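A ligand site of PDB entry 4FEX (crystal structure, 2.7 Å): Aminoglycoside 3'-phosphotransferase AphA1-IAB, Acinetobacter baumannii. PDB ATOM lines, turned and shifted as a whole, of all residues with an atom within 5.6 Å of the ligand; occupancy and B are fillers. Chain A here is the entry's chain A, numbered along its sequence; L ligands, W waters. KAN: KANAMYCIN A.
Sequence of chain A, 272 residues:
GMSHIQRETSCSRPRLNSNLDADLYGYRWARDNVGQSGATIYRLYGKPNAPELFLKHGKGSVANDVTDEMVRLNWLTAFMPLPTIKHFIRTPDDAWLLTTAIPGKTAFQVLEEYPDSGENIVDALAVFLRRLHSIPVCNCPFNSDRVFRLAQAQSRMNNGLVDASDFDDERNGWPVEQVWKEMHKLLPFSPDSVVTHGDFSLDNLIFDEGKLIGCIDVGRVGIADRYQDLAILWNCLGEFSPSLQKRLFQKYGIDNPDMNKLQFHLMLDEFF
The backbone carbonyl oxygen (O) of Asp 166 is in hydrogen-bond range of a nitrogen (N3) of the ligand (2.8 Å). The backbone carbonyl oxygen (O) of Phe 167 lies within hydrogen-bond range of an oxygen (O13) of the ligand, 3.5 Å away. The side-chain amide nitrogen (ND2) of Asn 235 lies within hydrogen-bond range of an oxygen (O14) of the ligand, at 3.1 Å. The side-chain carboxylate (OD2) of Asp 199 lies within hydrogen-bond range of an oxygen (O7) of the ligand, at 2.7 Å. The chain-end carboxylate (OXT) of Phe 272 lies within salt-bridge range of a nitrogen (N2) of the ligand, at 2.8 Å. The side-chain carboxylate (OE1) of Glu 270 is in salt-bridge range of a nitrogen (N3) of the ligand. The backbone NH (N) of Asp 168 sits close to a nitrogen (N3) of the ligand (3.4 Å). The backbone carbonyl oxygen (O) of Asp 269 is in hydrogen-bond range of a nitrogen (N2) of the ligand. The side-chain carboxylate of Asp 269 lies within salt-bridge range of a nitrogen (N2) of the ligand. The side-chain carboxylate of Asp 168 is in salt-bridge range of a nitrogen (N3) of the ligand, at 3.1 Å. O14 of the ligand sits at hydrogen-bond distance from OE1 of Glu 239, at 2.8 Å.
The side-chain carboxylate (OE2) of Glu 270 is in hydrogen-bond range of the backbone NH (N) of Asp 168. The chain-end carboxylate (O) of Phe 272 is in salt-bridge range of the guanidinium group (NH2) of Arg 156. The backbone carbonyl oxygen of Asp 199 lies within hydrogen-bond range of the side-chain amide nitrogen of Asn 204, 2.9 Å away. OD1 of Asp 168 is in hydrogen-bond range of ND2 of Asn 235, at 3.2 Å.
Ser 37 touches the ligand (OG to O8, 3.6 Å). Cys 236 touches the ligand. The nearest printed residue that does not touch the ligand is Arg 220 (4.3 Å).
Water W3 lies within hydrogen-bond range of OD2 of Asp 269 (2.9 Å), O6 of the ligand (3.0 Å) and OD1 of Asp 199 (3.1 Å). Water W2 lies within hydrogen-bond range of OD2 of Asp 168 (2.7 Å), O of Leu 266 (2.8 Å) and N3 of the ligand (3.5 Å). Water W1 bridges OD1 of Asp 169 (2.9 Å) and O13 of the ligand (3.5 Å).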
ATOM      1  N   GLY A  35     -20.704  -3.188  26.076  1.00  0.00           N
ATOM      2  CA  GLY A  35     -21.795  -4.000  25.565  1.00  0.00           C
ATOM      3  C   GLY A  35     -21.285  -5.353  25.114  1.00  0.00           C
ATOM      4  O   GLY A  35     -22.018  -6.154  24.524  1.00  0.00           O
ATOM      5  N   SER A  37     -20.373  -8.888  24.463  1.00  0.00           N
ATOM      6  CA  SER A  37     -20.940 -10.202  24.769  1.00  0.00           C
ATOM      7  C   SER A  37     -19.931 -11.107  25.465  1.00  0.00           C
ATOM      8  O   SER A  37     -18.980 -11.586  24.859  1.00  0.00           O
ATOM      9  CB  SER A  37     -21.425 -10.884  23.483  1.00  0.00           C
ATOM     10  OG  SER A  37     -22.338 -10.062  22.788  1.00  0.00           O
ATOM     11  N   ARG A 156     -28.708 -19.592  19.338  1.00  0.00           N
ATOM     12  CA  ARG A 156     -28.838 -18.584  20.393  1.00  0.00           C
ATOM     13  C   ARG A 156     -30.309 -18.303  20.643  1.00  0.00           C
ATOM     14  O   ARG A 156     -30.707 -17.914  21.752  1.00  0.00           O
ATOM     15  CB  ARG A 156     -28.088 -17.303  20.031  1.00  0.00           C
ATOM     16  CG  ARG A 156     -26.579 -17.485  19.929  1.00  0.00           C
ATOM     17  CD  ARG A 156     -25.874 -16.159  19.887  1.00  0.00           C
ATOM     18  NE  ARG A 156     -26.510 -15.202  20.797  1.00  0.00           N
ATOM     19  CZ  ARG A 156     -26.035 -13.992  21.065  1.00  0.00           C
ATOM     20  NH1 ARG A 156     -26.691 -13.200  21.891  1.00  0.00           N
ATOM     21  NH2 ARG A 156     -24.900 -13.585  20.505  1.00  0.00           N
ATOM     22  N   ASP A 163     -31.316 -11.049  22.545  1.00  0.00           N
ATOM     23  CA  ASP A 163     -31.816  -9.913  23.333  1.00  0.00           C
ATOM     24  C   ASP A 163     -32.969  -9.152  22.640  1.00  0.00           C
ATOM     25  O   ASP A 163     -32.749  -8.118  21.992  1.00  0.00           O
ATOM     26  CB  ASP A 163     -30.660  -8.981  23.699  1.00  0.00           C
ATOM     27  CG  ASP A 163     -31.092  -7.820  24.597  1.00  0.00           C
ATOM     28  OD1 ASP A 163     -32.235  -7.827  25.154  1.00  0.00           O
ATOM     29  OD2 ASP A 163     -30.269  -6.897  24.758  1.00  0.00           O
ATOM     30  N   ASP A 166     -33.420  -5.448  22.460  1.00  0.00           N
ATOM     31  CA  ASP A 166     -32.585  -4.588  21.617  1.00  0.00           C
ATOM     32  C   ASP A 166     -32.838  -4.660  20.111  1.00  0.00           C
ATOM     33  O   ASP A 166     -32.052  -4.139  19.321  1.00  0.00           O
ATOM     34  CB  ASP A 166     -31.107  -4.791  21.928  1.00  0.00           C
ATOM     35  CG  ASP A 166     -30.282  -3.618  21.484  1.00  0.00           C
ATOM     36  OD1 ASP A 166     -30.888  -2.534  21.300  1.00  0.00           O
ATOM     37  OD2 ASP A 166     -29.058  -3.774  21.273  1.00  0.00           O
ATOM     38  N   PHE A 167     -33.939  -5.278  19.718  1.00  0.00           N
ATOM     39  CA  PHE A 167     -34.344  -5.305  18.319  1.00  0.00           C
ATOM     40  C   PHE A 167     -34.423  -3.896  17.719  1.00  0.00           C
ATOM     41  O   PHE A 167     -34.653  -2.914  18.428  1.00  0.00           O
ATOM     42  CB  PHE A 167     -35.653  -6.052  18.151  1.00  0.00           C
ATOM     43  CG  PHE A 167     -35.560  -7.526  18.420  1.00  0.00           C
ATOM     44  CD1 PHE A 167     -34.348  -8.113  18.752  1.00  0.00           C
ATOM     45  CD2 PHE A 167     -36.679  -8.336  18.329  1.00  0.00           C
ATOM     46  CE1 PHE A 167     -34.265  -9.475  18.994  1.00  0.00           C
ATOM     47  CE2 PHE A 167     -36.588  -9.702  18.566  1.00  0.00           C
ATOM     48  CZ  PHE A 167     -35.396 -10.274  18.898  1.00  0.00           C
ATOM     49  N   ASP A 168     -34.205  -3.802  16.419  1.00  0.00           N
ATOM     50  CA  ASP A 168     -34.356  -2.527  15.735  1.00  0.00           C
ATOM     51  C   ASP A 168     -35.823  -2.108  15.889  1.00  0.00           C
ATOM     52  O   ASP A 168     -36.681  -2.957  16.167  1.00  0.00           O
ATOM     53  CB  ASP A 168     -33.942  -2.636  14.268  1.00  0.00           C
ATOM     54  CG  ASP A 168     -32.418  -2.691  14.075  1.00  0.00           C
ATOM     55  OD1 ASP A 168     -31.678  -2.059  14.865  1.00  0.00           O
ATOM     56  OD2 ASP A 168     -31.943  -3.373  13.156  1.00  0.00           O
ATOM     57  N   ASP A 169     -36.122  -0.818  15.723  1.00  0.00           N
ATOM     58  CA  ASP A 169     -37.487  -0.312  15.907  1.00  0.00           C
ATOM     59  C   ASP A 169     -38.549  -1.053  15.093  1.00  0.00           C
ATOM     60  O   ASP A 169     -39.556  -1.491  15.631  1.00  0.00           O
ATOM     61  CB  ASP A 169     -37.560   1.183  15.617  1.00  0.00           C
ATOM     62  CG  ASP A 169     -36.732   2.002  16.587  1.00  0.00           C
ATOM     63  OD1 ASP A 169     -36.296   1.443  17.622  1.00  0.00           O
ATOM     64  OD2 ASP A 169     -36.518   3.204  16.323  1.00  0.00           O
ATOM     65  N   ASP A 199     -18.956  -6.827  12.236  1.00  0.00           N
ATOM     66  CA  ASP A 199     -19.612  -5.910  13.144  1.00  0.00           C
ATOM     67  C   ASP A 199     -19.176  -4.492  12.849  1.00  0.00           C
ATOM     68  O   ASP A 199     -18.602  -3.811  13.689  1.00  0.00           O
ATOM     69  CB  ASP A 199     -19.289  -6.260  14.591  1.00  0.00           C
ATOM     70  CG  ASP A 199     -20.295  -5.658  15.578  1.00  0.00           C
ATOM     71  OD1 ASP A 199     -21.461  -5.430  15.170  1.00  0.00           O
ATOM     72  OD2 ASP A 199     -19.917  -5.427  16.749  1.00  0.00           O
ATOM     73  N   SER A 201     -19.961  -1.485  13.018  1.00  0.00           N
ATOM     74  CA  SER A 201     -20.831  -0.539  13.678  1.00  0.00           C
ATOM     75  C   SER A 201     -20.049   0.727  13.966  1.00  0.00           C
ATOM     76  O   SER A 201     -18.865   0.799  13.706  1.00  0.00           O
ATOM     77  CB  SER A 201     -21.336  -1.126  14.985  1.00  0.00           C
ATOM     78  OG  SER A 201     -20.336  -1.053  15.978  1.00  0.00           O
ATOM     79  N   ASP A 203     -19.290   1.933  16.707  1.00  0.00           N
ATOM     80  CA  ASP A 203     -18.497   1.777  17.919  1.00  0.00           C
ATOM     81  C   ASP A 203     -17.152   1.131  17.633  1.00  0.00           C
ATOM     82  O   ASP A 203     -16.226   1.220  18.448  1.00  0.00           O
ATOM     83  CB  ASP A 203     -19.247   0.941  18.964  1.00  0.00           C
ATOM     84  CG  ASP A 203     -20.520   1.621  19.447  1.00  0.00           C
ATOM     85  OD1 ASP A 203     -20.455   2.819  19.798  1.00  0.00           O
ATOM     86  OD2 ASP A 203     -21.583   0.957  19.466  1.00  0.00           O
ATOM     87  N   ASN A 204     -17.039   0.507  16.467  1.00  0.00           N
ATOM     88  CA  ASN A 204     -15.893  -0.330  16.174  1.00  0.00           C
ATOM     89  C   ASN A 204     -14.851   0.253  15.209  1.00  0.00           C
ATOM     90  O   ASN A 204     -13.877  -0.417  14.871  1.00  0.00           O
ATOM     91  CB  ASN A 204     -16.358  -1.683  15.687  1.00  0.00           C
ATOM     92  CG  ASN A 204     -16.888  -2.528  16.799  1.00  0.00           C
ATOM     93  OD1 ASN A 204     -16.605  -2.259  17.963  1.00  0.00           O
ATOM     94  ND2 ASN A 204     -17.651  -3.561  16.450  1.00  0.00           N
ATOM     95  N   ASP A 217     -12.615  -5.056  17.335  1.00  0.00           N
ATOM     96  CA  ASP A 217     -13.649  -6.063  17.528  1.00  0.00           C
ATOM     97  C   ASP A 217     -13.783  -7.024  16.343  1.00  0.00           C
ATOM     98  O   ASP A 217     -14.881  -7.216  15.785  1.00  0.00           O
ATOM     99  CB  ASP A 217     -14.979  -5.371  17.858  1.00  0.00           C
ATOM    100  CG  ASP A 217     -15.744  -6.092  18.920  1.00  0.00           C
ATOM    101  OD1 ASP A 217     -15.120  -6.380  19.969  1.00  0.00           O
ATOM    102  OD2 ASP A 217     -16.938  -6.398  18.691  1.00  0.00           O
ATOM    103  N   ARG A 220     -15.687 -11.594  14.378  1.00  0.00           N
ATOM    104  CA  ARG A 220     -16.581 -12.256  13.420  1.00  0.00           C
ATOM    105  C   ARG A 220     -16.079 -12.106  12.002  1.00  0.00           C
ATOM    106  O   ARG A 220     -16.796 -12.472  11.064  1.00  0.00           O
ATOM    107  CB  ARG A 220     -18.007 -11.683  13.484  1.00  0.00           C
ATOM    108  CG  ARG A 220     -18.648 -11.751  14.846  1.00  0.00           C
ATOM    109  CD  ARG A 220     -20.134 -12.105  14.753  1.00  0.00           C
ATOM    110  NE  ARG A 220     -20.728 -12.225  16.085  1.00  0.00           N
ATOM    111  CZ  ARG A 220     -21.134 -11.192  16.813  1.00  0.00           C
ATOM    112  NH1 ARG A 220     -21.645 -11.401  18.026  1.00  0.00           N
ATOM    113  NH2 ARG A 220     -21.031  -9.955  16.345  1.00  0.00           N
ATOM    114  N   ASN A 235     -27.505   1.071   9.260  1.00  0.00           N
ATOM    115  CA  ASN A 235     -28.379   1.149  10.420  1.00  0.00           C
ATOM    116  C   ASN A 235     -27.845   2.144  11.459  1.00  0.00           C
ATOM    117  O   ASN A 235     -28.555   3.012  11.920  1.00  0.00           O
ATOM    118  CB  ASN A 235     -28.507  -0.238  11.031  1.00  0.00           C
ATOM    119  CG  ASN A 235     -29.724  -0.396  11.917  1.00  0.00           C
ATOM    120  OD1 ASN A 235     -30.836  -0.570  11.435  1.00  0.00           O
ATOM    121  ND2 ASN A 235     -29.506  -0.357  13.220  1.00  0.00           N
ATOM    122  N   CYS A 236     -26.586   2.026  11.834  1.00  0.00           N
ATOM    123  CA  CYS A 236     -26.032   2.972  12.772  1.00  0.00           C
ATOM    124  C   CYS A 236     -26.203   4.410  12.298  1.00  0.00           C
ATOM    125  O   CYS A 236     -26.452   5.301  13.107  1.00  0.00           O
ATOM    126  CB  CYS A 236     -24.557   2.684  13.024  1.00  0.00           C
ATOM    127  SG  CYS A 236     -24.267   1.120  13.818  1.00  0.00           S
ATOM    128  N   GLU A 239     -29.429   6.673  12.952  1.00  0.00           N
ATOM    129  CA  GLU A 239     -29.587   7.530  14.113  1.00  0.00           C
ATOM    130  C   GLU A 239     -29.080   8.945  13.878  1.00  0.00           C
ATOM    131  O   GLU A 239     -28.947   9.714  14.823  1.00  0.00           O
ATOM    132  CB  GLU A 239     -28.851   6.963  15.319  1.00  0.00           C
ATOM    133  CG  GLU A 239     -29.066   5.474  15.560  1.00  0.00           C
ATOM    134  CD  GLU A 239     -28.072   4.919  16.572  1.00  0.00           C
ATOM    135  OE1 GLU A 239     -27.232   4.059  16.172  1.00  0.00           O
ATOM    136  OE2 GLU A 239     -28.097   5.360  17.753  1.00  0.00           O
ATOM    137  N   LEU A 266     -29.705  -6.988   8.701  1.00  0.00           N
ATOM    138  CA  LEU A 266     -30.185  -6.323   9.905  1.00  0.00           C
ATOM    139  C   LEU A 266     -30.999  -7.278  10.762  1.00  0.00           C
ATOM    140  O   LEU A 266     -30.882  -7.270  11.985  1.00  0.00           O
ATOM    141  CB  LEU A 266     -30.997  -5.097   9.524  1.00  0.00           C
ATOM    142  CG  LEU A 266     -30.084  -3.946   9.155  1.00  0.00           C
ATOM    143  CD1 LEU A 266     -30.881  -2.685   8.913  1.00  0.00           C
ATOM    144  CD2 LEU A 266     -29.030  -3.769  10.228  1.00  0.00           C
ATOM    145  N   ASP A 269     -28.597  -9.633  12.529  1.00  0.00           N
ATOM    146  CA  ASP A 269     -27.832  -9.039  13.621  1.00  0.00           C
ATOM    147  C   ASP A 269     -28.648  -9.032  14.918  1.00  0.00           C
ATOM    148  O   ASP A 269     -28.103  -9.060  16.024  1.00  0.00           O
ATOM    149  CB  ASP A 269     -27.364  -7.637  13.237  1.00  0.00           C
ATOM    150  CG  ASP A 269     -26.209  -7.141  14.110  1.00  0.00           C
ATOM    151  OD1 ASP A 269     -25.447  -7.989  14.621  1.00  0.00           O
ATOM    152  OD2 ASP A 269     -26.072  -5.909  14.289  1.00  0.00           O
ATOM    153  N   GLU A 270     -29.966  -9.017  14.772  1.00  0.00           N
ATOM    154  CA  GLU A 270     -30.889  -9.003  15.906  1.00  0.00           C
ATOM    155  C   GLU A 270     -30.581 -10.139  16.855  1.00  0.00           C
ATOM    156  O   GLU A 270     -30.776 -10.000  18.065  1.00  0.00           O
ATOM    157  CB  GLU A 270     -32.348  -9.116  15.441  1.00  0.00           C
ATOM    158  CG  GLU A 270     -32.843  -7.985  14.531  1.00  0.00           C
ATOM    159  CD  GLU A 270     -33.034  -6.659  15.260  1.00  0.00           C
ATOM    160  OE1 GLU A 270     -32.336  -6.417  16.265  1.00  0.00           O
ATOM    161  OE2 GLU A 270     -33.890  -5.857  14.812  1.00  0.00           O
ATOM    162  N   PHE A 271     -30.109 -11.253  16.298  1.00  0.00           N
ATOM    163  CA  PHE A 271     -29.864 -12.486  17.028  1.00  0.00           C
ATOM    164  C   PHE A 271     -28.495 -12.554  17.696  1.00  0.00           C
ATOM    165  O   PHE A 271     -28.084 -13.598  18.196  1.00  0.00           O
ATOM    166  CB  PHE A 271     -29.948 -13.674  16.082  1.00  0.00           C
ATOM    167  CG  PHE A 271     -31.320 -13.968  15.577  1.00  0.00           C
ATOM    168  CD1 PHE A 271     -31.839 -13.247  14.528  1.00  0.00           C
ATOM    169  CD2 PHE A 271     -32.053 -15.003  16.129  1.00  0.00           C
ATOM    170  CE1 PHE A 271     -33.104 -13.530  14.051  1.00  0.00           C
ATOM    171  CE2 PHE A 271     -33.312 -15.284  15.659  1.00  0.00           C
ATOM    172  CZ  PHE A 271     -33.837 -14.550  14.613  1.00  0.00           C
ATOM    173  N   PHE A 272     -27.747 -11.460  17.689  1.00  0.00           N
ATOM    174  CA  PHE A 272     -26.394 -11.537  18.201  1.00  0.00           C
ATOM    175  C   PHE A 272     -26.141 -10.426  19.204  1.00  0.00           C
ATOM    176  O   PHE A 272     -25.103 -10.440  19.878  1.00  0.00           O
ATOM    177  CB  PHE A 272     -25.362 -11.495  17.070  1.00  0.00           C
ATOM    178  CG  PHE A 272     -25.380 -12.719  16.180  1.00  0.00           C
ATOM    179  CD1 PHE A 272     -26.227 -12.782  15.083  1.00  0.00           C
ATOM    180  CD2 PHE A 272     -24.543 -13.791  16.432  1.00  0.00           C
ATOM    181  CE1 PHE A 272     -26.246 -13.895  14.265  1.00  0.00           C
ATOM    182  CE2 PHE A 272     -24.556 -14.916  15.612  1.00  0.00           C
ATOM    183  CZ  PHE A 272     -25.404 -14.974  14.528  1.00  0.00           C
ATOM    184  OXT PHE A 272     -26.968  -9.519  19.347  1.00  0.00           O
HETATM  185  C1  KAN L   1     -24.918  -4.245  19.744  1.00  0.00           C
HETATM  186  C2  KAN L   1     -23.394  -4.198  19.506  1.00  0.00           C
HETATM  187  C3  KAN L   1     -22.823  -5.584  19.208  1.00  0.00           C
HETATM  188  C4  KAN L   1     -23.145  -6.513  20.346  1.00  0.00           C
HETATM  189  C5  KAN L   1     -24.668  -6.596  20.483  1.00  0.00           C
HETATM  190  C6  KAN L   1     -25.026  -7.685  21.510  1.00  0.00           C
HETATM  191  C7  KAN L   1     -29.436  -4.335  16.831  1.00  0.00           C
HETATM  192  C8  KAN L   1     -29.037  -3.280  17.814  1.00  0.00           C
HETATM  193  C9  KAN L   1     -27.479  -3.341  17.899  1.00  0.00           C
HETATM  194  C10 KAN L   1     -27.008  -4.675  18.495  1.00  0.00           C
HETATM  195  C11 KAN L   1     -27.450  -5.726  17.469  1.00  0.00           C
HETATM  196  C12 KAN L   1     -28.944  -5.693  17.310  1.00  0.00           C
HETATM  197  C13 KAN L   1     -29.614  -0.991  18.196  1.00  0.00           C
HETATM  198  C14 KAN L   1     -30.720  -0.077  17.685  1.00  0.00           C
HETATM  199  C15 KAN L   1     -30.425   0.501  16.334  1.00  0.00           C
HETATM  200  C16 KAN L   1     -29.136   1.318  16.505  1.00  0.00           C
HETATM  201  C17 KAN L   1     -28.049   0.395  16.979  1.00  0.00           C
HETATM  202  C18 KAN L   1     -26.824   1.302  17.187  1.00  0.00           C
HETATM  203  N1  KAN L   1     -26.491  -7.764  21.598  1.00  0.00           N
HETATM  204  N2  KAN L   1     -27.129  -7.048  18.019  1.00  0.00           N
HETATM  205  N3  KAN L   1     -30.909  -4.350  16.729  1.00  0.00           N
HETATM  206  N4  KAN L   1     -31.589   1.313  15.932  1.00  0.00           N
HETATM  207  O5  KAN L   1     -25.183  -5.236  20.765  1.00  0.00           O
HETATM  208  O6  KAN L   1     -23.061  -3.371  18.392  1.00  0.00           O
HETATM  209  O7  KAN L   1     -21.404  -5.530  19.057  1.00  0.00           O
HETATM  210  O8  KAN L   1     -22.605  -7.790  20.066  1.00  0.00           O
HETATM  211  O9  KAN L   1     -25.564  -4.779  18.579  1.00  0.00           O
HETATM  212  O10 KAN L   1     -26.880  -2.225  18.582  1.00  0.00           O
HETATM  213  O11 KAN L   1     -29.569  -2.069  17.265  1.00  0.00           O
HETATM  214  O12 KAN L   1     -28.391  -0.209  18.230  1.00  0.00           O
HETATM  215  O13 KAN L   1     -31.920  -0.876  17.674  1.00  0.00           O
HETATM  216  O14 KAN L   1     -28.761   1.906  15.255  1.00  0.00           O
HETATM  217  O15 KAN L   1     -25.721   0.518  17.635  1.00  0.00           O
HETATM  218  O   HOH W   1     -34.003   1.344  19.315  1.00  0.00           O
HETATM  219  O   HOH W   2     -29.888  -5.118  13.499  1.00  0.00           O
HETATM  220  O   HOH W   3     -24.308  -4.232  15.786  1.00  0.00           O
